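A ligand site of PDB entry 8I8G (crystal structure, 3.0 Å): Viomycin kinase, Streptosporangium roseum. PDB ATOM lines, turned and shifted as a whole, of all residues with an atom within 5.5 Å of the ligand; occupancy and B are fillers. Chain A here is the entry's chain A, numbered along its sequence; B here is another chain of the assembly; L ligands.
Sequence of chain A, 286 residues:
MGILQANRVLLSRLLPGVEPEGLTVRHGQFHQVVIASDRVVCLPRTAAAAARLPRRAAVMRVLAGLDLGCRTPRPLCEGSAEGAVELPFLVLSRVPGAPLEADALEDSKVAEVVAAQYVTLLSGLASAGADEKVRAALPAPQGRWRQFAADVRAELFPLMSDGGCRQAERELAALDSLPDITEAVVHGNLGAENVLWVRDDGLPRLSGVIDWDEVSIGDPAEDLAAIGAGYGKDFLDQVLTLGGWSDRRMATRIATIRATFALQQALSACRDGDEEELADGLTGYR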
ATOM      1  N   ARG A  26     -23.338  -2.637  18.297  1.00  0.00           N
ATOM      2  CA  ARG A  26     -22.020  -2.946  17.768  1.00  0.00           C
ATOM      3  C   ARG A  26     -22.170  -3.954  16.639  1.00  0.00           C
ATOM      4  O   ARG A  26     -22.253  -5.159  16.864  1.00  0.00           O
ATOM      5  CB  ARG A  26     -21.102  -3.470  18.893  1.00  0.00           C
ATOM      6  CG  ARG A  26     -20.896  -2.491  20.034  1.00  0.00           C
ATOM      7  CD  ARG A  26     -20.187  -1.218  19.623  1.00  0.00           C
ATOM      8  NE  ARG A  26     -20.057  -0.272  20.720  1.00  0.00           N
ATOM      9  CZ  ARG A  26     -19.573   0.963  20.611  1.00  0.00           C
ATOM     10  NH1 ARG A  26     -19.511   1.752  21.663  1.00  0.00           N
ATOM     11  NH2 ARG A  26     -19.141   1.391  19.437  1.00  0.00           N
ATOM     12  N   GLY A  28     -21.025  -6.250  14.506  1.00  0.00           N
ATOM     13  CA  GLY A  28     -19.883  -7.135  14.358  1.00  0.00           C
ATOM     14  C   GLY A  28     -19.901  -7.872  13.021  1.00  0.00           C
ATOM     15  O   GLY A  28     -20.553  -7.429  12.078  1.00  0.00           O
ATOM     16  N   GLN A  29     -19.189  -8.999  12.960  1.00  0.00           N
ATOM     17  CA  GLN A  29     -19.013  -9.749  11.736  1.00  0.00           C
ATOM     18  C   GLN A  29     -20.269 -10.575  11.448  1.00  0.00           C
ATOM     19  O   GLN A  29     -20.916 -10.388  10.422  1.00  0.00           O
ATOM     20  CB  GLN A  29     -17.779 -10.652  11.819  1.00  0.00           C
ATOM     21  CG  GLN A  29     -16.486  -9.881  12.061  1.00  0.00           C
ATOM     22  CD  GLN A  29     -15.265 -10.767  12.032  1.00  0.00           C
ATOM     23  OE1 GLN A  29     -15.351 -11.973  11.796  1.00  0.00           O
ATOM     24  NE2 GLN A  29     -14.103 -10.166  12.273  1.00  0.00           N
ATOM     25  N   PHE A  30     -20.596 -11.488  12.378  1.00  0.00           N
ATOM     26  CA  PHE A  30     -21.687 -12.438  12.196  1.00  0.00           C
ATOM     27  C   PHE A  30     -22.958 -11.958  12.894  1.00  0.00           C
ATOM     28  O   PHE A  30     -24.046 -12.118  12.349  1.00  0.00           O
ATOM     29  CB  PHE A  30     -21.272 -13.819  12.708  1.00  0.00           C
ATOM     30  CG  PHE A  30     -20.135 -14.470  11.958  1.00  0.00           C
ATOM     31  CD1 PHE A  30     -20.244 -14.713  10.599  1.00  0.00           C
ATOM     32  CD2 PHE A  30     -18.973 -14.835  12.614  1.00  0.00           C
ATOM     33  CE1 PHE A  30     -19.190 -15.313   9.912  1.00  0.00           C
ATOM     34  CE2 PHE A  30     -17.930 -15.427  11.923  1.00  0.00           C
ATOM     35  CZ  PHE A  30     -18.039 -15.670  10.565  1.00  0.00           C
ATOM     36  N   HIS A  31     -22.814 -11.394  14.090  1.00  0.00           N
ATOM     37  CA  HIS A  31     -23.953 -11.053  14.930  1.00  0.00           C
ATOM     38  C   HIS A  31     -24.088  -9.530  15.069  1.00  0.00           C
ATOM     39  O   HIS A  31     -23.121  -8.795  14.875  1.00  0.00           O
ATOM     40  CB  HIS A  31     -23.834 -11.722  16.304  1.00  0.00           C
ATOM     41  CG  HIS A  31     -23.774 -13.215  16.240  1.00  0.00           C
ATOM     42  ND1 HIS A  31     -22.692 -13.934  16.706  1.00  0.00           N
ATOM     43  CD2 HIS A  31     -24.646 -14.107  15.760  1.00  0.00           C
ATOM     44  CE1 HIS A  31     -22.924 -15.226  16.510  1.00  0.00           C
ATOM     45  NE2 HIS A  31     -24.104 -15.352  15.934  1.00  0.00           N
ATOM     46  N   GLN A  32     -25.315  -9.096  15.391  1.00  0.00           N
ATOM     47  CA  GLN A  32     -25.605  -7.708  15.706  1.00  0.00           C
ATOM     48  C   GLN A  32     -25.992  -7.614  17.179  1.00  0.00           C
ATOM     49  O   GLN A  32     -27.156  -7.851  17.532  1.00  0.00           O
ATOM     50  CB  GLN A  32     -26.753  -7.194  14.830  1.00  0.00           C
ATOM     51  CG  GLN A  32     -26.349  -6.914  13.396  1.00  0.00           C
ATOM     52  CD  GLN A  32     -25.658  -5.584  13.224  1.00  0.00           C
ATOM     53  OE1 GLN A  32     -25.576  -4.776  14.148  1.00  0.00           O
ATOM     54  NE2 GLN A  32     -25.166  -5.332  12.014  1.00  0.00           N
ATOM     55  N   VAL A  33     -25.026  -7.270  18.041  1.00  0.00           N
ATOM     56  CA  VAL A  33     -25.247  -7.230  19.473  1.00  0.00           C
ATOM     57  C   VAL A  33     -25.766  -5.852  19.867  1.00  0.00           C
ATOM     58  O   VAL A  33     -25.150  -4.838  19.544  1.00  0.00           O
ATOM     59  CB  VAL A  33     -23.976  -7.612  20.261  1.00  0.00           C
ATOM     60  CG1 VAL A  33     -23.486  -9.011  19.879  1.00  0.00           C
ATOM     61  CG2 VAL A  33     -22.856  -6.604  20.105  1.00  0.00           C
ATOM     62  N   ILE A  35     -26.316  -3.313  22.716  1.00  0.00           N
ATOM     63  CA  ILE A  35     -25.689  -3.069  23.996  1.00  0.00           C
ATOM     64  C   ILE A  35     -26.698  -2.387  24.930  1.00  0.00           C
ATOM     65  O   ILE A  35     -27.026  -1.220  24.738  1.00  0.00           O
ATOM     66  CB  ILE A  35     -24.399  -2.226  23.836  1.00  0.00           C
ATOM     67  CG1 ILE A  35     -23.446  -2.842  22.805  1.00  0.00           C
ATOM     68  CG2 ILE A  35     -23.729  -2.004  25.183  1.00  0.00           C
ATOM     69  CD1 ILE A  35     -23.035  -4.260  23.109  1.00  0.00           C
ATOM     70  N   VAL A  40     -26.516  -7.798  26.645  1.00  0.00           N
ATOM     71  CA  VAL A  40     -26.479  -7.601  25.206  1.00  0.00           C
ATOM     72  C   VAL A  40     -27.424  -8.605  24.548  1.00  0.00           C
ATOM     73  O   VAL A  40     -27.770  -9.612  25.156  1.00  0.00           O
ATOM     74  CB  VAL A  40     -25.037  -7.738  24.651  1.00  0.00           C
ATOM     75  CG1 VAL A  40     -24.096  -6.732  25.295  1.00  0.00           C
ATOM     76  CG2 VAL A  40     -24.493  -9.156  24.804  1.00  0.00           C
ATOM     77  N   CYS A  42     -27.651 -10.734  21.106  1.00  0.00           N
ATOM     78  CA  CYS A  42     -27.069 -11.218  19.861  1.00  0.00           C
ATOM     79  C   CYS A  42     -28.163 -11.538  18.859  1.00  0.00           C
ATOM     80  O   CYS A  42     -29.133 -12.215  19.192  1.00  0.00           O
ATOM     81  CB  CYS A  42     -26.208 -12.454  20.095  1.00  0.00           C
ATOM     82  SG  CYS A  42     -24.738 -12.124  21.107  1.00  0.00           S
ATOM     83  N   PRO A  73     -19.901 -13.926  29.462  1.00  0.00           N
ATOM     84  CA  PRO A  73     -21.293 -13.657  29.073  1.00  0.00           C
ATOM     85  C   PRO A  73     -22.184 -14.873  29.309  1.00  0.00           C
ATOM     86  O   PRO A  73     -22.059 -15.892  28.630  1.00  0.00           O
ATOM     87  CB  PRO A  73     -21.222 -13.284  27.580  1.00  0.00           C
ATOM     88  CG  PRO A  73     -19.809 -13.583  27.124  1.00  0.00           C
ATOM     89  CD  PRO A  73     -18.953 -13.682  28.365  1.00  0.00           C
ATOM     90  N   LEU A  92     -27.156 -12.251  26.359  1.00  0.00           N
ATOM     91  CA  LEU A  92     -25.985 -12.567  27.158  1.00  0.00           C
ATOM     92  C   LEU A  92     -25.749 -11.466  28.188  1.00  0.00           C
ATOM     93  O   LEU A  92     -26.114 -10.311  27.945  1.00  0.00           O
ATOM     94  CB  LEU A  92     -24.770 -12.716  26.234  1.00  0.00           C
ATOM     95  CG  LEU A  92     -24.866 -13.805  25.169  1.00  0.00           C
ATOM     96  CD1 LEU A  92     -23.556 -13.928  24.408  1.00  0.00           C
ATOM     97  CD2 LEU A  92     -25.237 -15.146  25.796  1.00  0.00           C
ATOM     98  N   SER A  93     -25.147 -11.832  29.322  1.00  0.00           N
ATOM     99  CA  SER A  93     -24.806 -10.861  30.348  1.00  0.00           C
ATOM    100  C   SER A  93     -23.654  -9.986  29.874  1.00  0.00           C
ATOM    101  O   SER A  93     -22.760 -10.467  29.168  1.00  0.00           O
ATOM    102  CB  SER A  93     -24.476 -11.548  31.660  1.00  0.00           C
ATOM    103  OG  SER A  93     -23.263 -12.287  31.555  1.00  0.00           O
ATOM    104  N   ARG A  94     -23.690  -8.700  30.247  1.00  0.00           N
ATOM    105  CA  ARG A  94     -22.672  -7.748  29.852  1.00  0.00           C
ATOM    106  C   ARG A  94     -21.581  -7.725  30.924  1.00  0.00           C
ATOM    107  O   ARG A  94     -21.830  -7.302  32.056  1.00  0.00           O
ATOM    108  CB  ARG A  94     -23.274  -6.360  29.667  1.00  0.00           C
ATOM    109  CG  ARG A  94     -22.318  -5.320  29.108  1.00  0.00           C
ATOM    110  CD  ARG A  94     -22.946  -3.939  29.038  1.00  0.00           C
ATOM    111  NE  ARG A  94     -22.029  -2.929  28.529  1.00  0.00           N
ATOM    112  CZ  ARG A  94     -22.320  -1.635  28.438  1.00  0.00           C
ATOM    113  NH1 ARG A  94     -23.500  -1.189  28.816  1.00  0.00           N
ATOM    114  NH2 ARG A  94     -21.423  -0.793  27.959  1.00  0.00           N
ATOM    115  N   VAL A  95     -20.381  -8.199  30.560  1.00  0.00           N
ATOM    116  CA  VAL A  95     -19.238  -8.195  31.462  1.00  0.00           C
ATOM    117  C   VAL A  95     -18.828  -6.738  31.697  1.00  0.00           C
ATOM    118  O   VAL A  95     -18.530  -6.027  30.744  1.00  0.00           O
ATOM    119  CB  VAL A  95     -18.069  -9.027  30.887  1.00  0.00           C
ATOM    120  CG1 VAL A  95     -16.819  -8.925  31.752  1.00  0.00           C
ATOM    121  CG2 VAL A  95     -18.471 -10.479  30.694  1.00  0.00           C
ATOM    122  N   GLU A 193      -8.865  -5.901  23.928  1.00  0.00           N
ATOM    123  CA  GLU A 193     -10.167  -5.261  24.044  1.00  0.00           C
ATOM    124  C   GLU A 193     -11.234  -6.270  24.451  1.00  0.00           C
ATOM    125  O   GLU A 193     -12.327  -5.869  24.853  1.00  0.00           O
ATOM    126  CB  GLU A 193     -10.536  -4.534  22.747  1.00  0.00           C
ATOM    127  CG  GLU A 193     -11.039  -5.434  21.624  1.00  0.00           C
ATOM    128  CD  GLU A 193      -9.989  -6.299  20.943  1.00  0.00           C
ATOM    129  OE1 GLU A 193      -8.791  -6.143  21.262  1.00  0.00           O
ATOM    130  OE2 GLU A 193     -10.372  -7.111  20.079  1.00  0.00           O
ATOM    131  N   ASN A 194     -10.933  -7.567  24.342  1.00  0.00           N
ATOM    132  CA  ASN A 194     -11.855  -8.628  24.721  1.00  0.00           C
ATOM    133  C   ASN A 194     -11.702  -8.982  26.196  1.00  0.00           C
ATOM    134  O   ASN A 194     -12.563  -9.660  26.752  1.00  0.00           O
ATOM    135  CB  ASN A 194     -11.682  -9.872  23.850  1.00  0.00           C
ATOM    136  CG  ASN A 194     -12.117  -9.660  22.413  1.00  0.00           C
ATOM    137  OD1 ASN A 194     -13.259  -9.299  22.155  1.00  0.00           O
ATOM    138  ND2 ASN A 194     -11.225  -9.900  21.472  1.00  0.00           N
ATOM    139  N   LEU A 196     -11.669  -7.528  29.902  1.00  0.00           N
ATOM    140  CA  LEU A 196     -12.158  -6.342  30.589  1.00  0.00           C
ATOM    141  C   LEU A 196     -11.661  -6.350  32.033  1.00  0.00           C
ATOM    142  O   LEU A 196     -11.494  -7.413  32.638  1.00  0.00           O
ATOM    143  CB  LEU A 196     -13.687  -6.336  30.526  1.00  0.00           C
ATOM    144  CG  LEU A 196     -14.287  -6.477  29.127  1.00  0.00           C
ATOM    145  CD1 LEU A 196     -15.798  -6.285  29.162  1.00  0.00           C
ATOM    146  CD2 LEU A 196     -13.652  -5.497  28.150  1.00  0.00           C
ATOM    147  N   ILE A 210     -14.804 -11.714  26.980  1.00  0.00           N
ATOM    148  CA  ILE A 210     -15.978 -11.725  26.070  1.00  0.00           C
ATOM    149  C   ILE A 210     -15.513 -12.084  24.664  1.00  0.00           C
ATOM    150  O   ILE A 210     -14.291 -12.119  24.448  1.00  0.00           O
ATOM    151  CB  ILE A 210     -16.667 -10.345  26.096  1.00  0.00           C
ATOM    152  CG1 ILE A 210     -15.709  -9.227  25.685  1.00  0.00           C
ATOM    153  CG2 ILE A 210     -17.283 -10.069  27.457  1.00  0.00           C
ATOM    154  CD1 ILE A 210     -16.365  -8.122  24.900  1.00  0.00           C
ATOM    155  N   ASP A 211     -16.443 -12.335  23.746  1.00  0.00           N
ATOM    156  CA  ASP A 211     -16.129 -12.679  22.328  1.00  0.00           C
ATOM    157  C   ASP A 211     -15.582 -14.097  22.252  1.00  0.00           C
ATOM    158  O   ASP A 211     -14.381 -14.260  22.078  1.00  0.00           O
ATOM    159  CB  ASP A 211     -15.223 -11.636  21.679  1.00  0.00           C
ATOM    160  CG  ASP A 211     -15.284 -11.671  20.164  1.00  0.00           C
ATOM    161  OD1 ASP A 211     -16.064 -12.478  19.635  1.00  0.00           O
ATOM    162  OD2 ASP A 211     -14.544 -10.894  19.533  1.00  0.00           O
ATOM    163  N   ASP A 213     -16.550 -16.431  19.875  1.00  0.00           N
ATOM    164  CA  ASP A 213     -17.080 -16.914  18.609  1.00  0.00           C
ATOM    165  C   ASP A 213     -16.071 -17.842  17.932  1.00  0.00           C
ATOM    166  O   ASP A 213     -16.453 -18.646  17.083  1.00  0.00           O
ATOM    167  CB  ASP A 213     -17.483 -15.762  17.700  1.00  0.00           C
ATOM    168  CG  ASP A 213     -18.775 -15.082  18.126  1.00  0.00           C
ATOM    169  OD1 ASP A 213     -18.795 -14.503  19.241  1.00  0.00           O
ATOM    170  OD2 ASP A 213     -19.759 -15.143  17.361  1.00  0.00           O
ATOM    171  N   GLU A 214     -14.795 -17.729  18.307  1.00  0.00           N
ATOM    172  CA  GLU A 214     -13.743 -18.562  17.747  1.00  0.00           C
ATOM    173  C   GLU A 214     -13.281 -19.595  18.780  1.00  0.00           C
ATOM    174  O   GLU A 214     -12.156 -20.089  18.704  1.00  0.00           O
ATOM    175  CB  GLU A 214     -12.573 -17.677  17.300  1.00  0.00           C
ATOM    176  CG  GLU A 214     -12.947 -16.667  16.227  1.00  0.00           C
ATOM    177  CD  GLU A 214     -11.836 -15.705  15.855  1.00  0.00           C
ATOM    178  OE1 GLU A 214     -12.050 -14.487  15.941  1.00  0.00           O
ATOM    179  OE2 GLU A 214     -10.741 -16.185  15.487  1.00  0.00           O
ATOM    180  C   KBE B   1     -10.827  -6.595  14.163  1.00  0.00           C
ATOM    181  N   KBE B   1     -14.415  -5.270  14.368  1.00  0.00           N
ATOM    182  O   KBE B   1     -10.938  -7.509  14.943  1.00  0.00           O
ATOM    183  CA  KBE B   1     -12.269  -6.265  13.595  1.00  0.00           C
ATOM    184  CB  KBE B   1     -13.404  -6.296  14.640  1.00  0.00           C
ATOM    185  CD  KBE B   1     -14.637  -8.048  16.081  1.00  0.00           C
ATOM    186  CE  KBE B   1     -13.635  -8.851  16.895  1.00  0.00           C
ATOM    187  CG  KBE B   1     -14.063  -7.675  14.718  1.00  0.00           C
ATOM    188  NZ  KBE B   1     -13.821  -8.637  18.346  1.00  0.00           N
HETATM  189  P1  LIG L   1     -17.235 -12.122  15.722  1.00  0.00           P
HETATM  190  O1  LIG L   1     -16.646 -12.504  17.049  1.00  0.00           O
HETATM  191  O2  LIG L   1     -17.002 -13.157  14.655  1.00  0.00           O
HETATM  192  O3  LIG L   1     -16.824 -10.730  15.283  1.00  0.00           O
HETATM  193  P2  LIG L   1     -19.799 -11.108  16.786  1.00  0.00           P
HETATM  194  O4  LIG L   1     -20.562 -10.250  15.830  1.00  0.00           O
HETATM  195  O5  LIG L   1     -20.543 -11.931  17.786  1.00  0.00           O
HETATM  196  O6  LIG L   1     -18.831 -12.068  15.939  1.00  0.00           O
HETATM  197  P3  LIG L   1     -18.857  -9.380  18.944  1.00  0.00           P
HETATM  198  O7  LIG L   1     -18.111 -10.134  19.997  1.00  0.00           O
HETATM  199  O8  LIG L   1     -20.289  -9.061  19.202  1.00  0.00           O
HETATM  200  O9  LIG L   1     -18.744 -10.181  17.568  1.00  0.00           O
HETATM  201  O10 LIG L   1     -18.068  -8.024  18.597  1.00  0.00           O
HETATM  202  C1  LIG L   1     -17.145  -7.446  19.547  1.00  0.00           C
HETATM  203  C2  LIG L   1     -17.834  -6.337  20.320  1.00  0.00           C
HETATM  204  O11 LIG L   1     -19.146  -6.783  20.744  1.00  0.00           O
HETATM  205  C3  LIG L   1     -17.134  -5.899  21.611  1.00  0.00           C
HETATM  206  O12 LIG L   1     -16.153  -4.906  21.341  1.00  0.00           O
HETATM  207  C4  LIG L   1     -18.301  -5.351  22.430  1.00  0.00           C
HETATM  208  O13 LIG L   1     -18.575  -3.998  22.151  1.00  0.00           O
HETATM  209  C5  LIG L   1     -19.461  -6.244  22.009  1.00  0.00           C
HETATM  210  N1  LIG L   1     -19.754  -7.356  22.928  1.00  0.00           N
HETATM  211  C6  LIG L   1     -19.915  -8.693  22.614  1.00  0.00           C
HETATM  212  N2  LIG L   1     -20.170  -9.422  23.672  1.00  0.00           N
HETATM  213  C7  LIG L   1     -20.198  -8.531  24.730  1.00  0.00           C
HETATM  214  C8  LIG L   1     -20.430  -8.694  26.112  1.00  0.00           C
HETATM  215  N3  LIG L   1     -20.681  -9.869  26.683  1.00  0.00           N
HETATM  216  N4  LIG L   1     -20.379  -7.585  26.889  1.00  0.00           N
HETATM  217  C9  LIG L   1     -20.123  -6.408  26.309  1.00  0.00           C
HETATM  218  N5  LIG L   1     -19.895  -6.137  25.021  1.00  0.00           N
HETATM  219  C10 LIG L   1     -19.944  -7.252  24.279  1.00  0.00           C
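An oxygen (O1) of the ligand sits close to the side-chain carboxylate of Asp 211.
An oxygen (O4) of the ligand is in hydrogen-bond range of the backbone NH (N) of His 31, at 3.1 Å.
O of His 31 lies close to O4 of the ligand (3.1 Å).
A ring nitrogen (ND1) of His 31 sits at hydrogen-bond distance from an oxygen (O5) of the ligand (3.1 Å).
The backbone carbonyl oxygen of Ser 93 lies within hydrogen-bond range of a nitrogen (N3) of the ligand (3.3 Å).
The backbone NH (N) of Gln 29 sits at hydrogen-bond distance from an oxygen (O4) of the ligand, at 3.4 Å.
The side-chain carboxylate (OD2) of Asp 211 lies within salt-bridge range of NZ of KBE 1 of chain B (2.7 Å).
OD2 of Asp 211 sits close to OD1 of Asn 194 (3.3 Å).
OD2 of Asp 213 lies within hydrogen-bond range of ND1 of His 31 (3.2 Å).
The backbone carbonyl oxygen (O) of Val 33 sits at hydrogen-bond distance from the backbone NH (N) of Arg 26 (3.1 Å).
The backbone NH (N) of Ile 210 sits at hydrogen-bond distance from the backbone carbonyl oxygen (O) of Asn 194 (3.0 Å).
The side-chain carboxylate of Asp 213 sits close to an oxygen (O5) of the ligand.
Arg 26 touches the ligand.
Gly 28 touches the ligand.
CD2 of Phe 30 touches O2 of the ligand (3.3 Å).
Val 33 touches the ligand.
CB of Pro 73 touches N3 of the ligand, at 3.6 Å.
CG of Arg 94 touches N4 of the ligand, at 3.7 Å.
Val 95 touches the ligand (N to N4, 3.7 Å).
CG2 of Ile 210 touches N3 of the ligand (3.5 Å).
KBE 1 of chain B touches the ligand.
Hydrophobic or aromatic side chains within 4 Å of the ligand: Phe 30, His 31, Val 33, Pro 73 and Ile 210.
Of the 23 residues printed, 14 come within 4 Å of the ligand.
Along chain A the residues within 4 Å of the ligand span positions 26 to 213.
The nearest printed residue that does not touch the ligand is Val 40 (4.1 Å).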
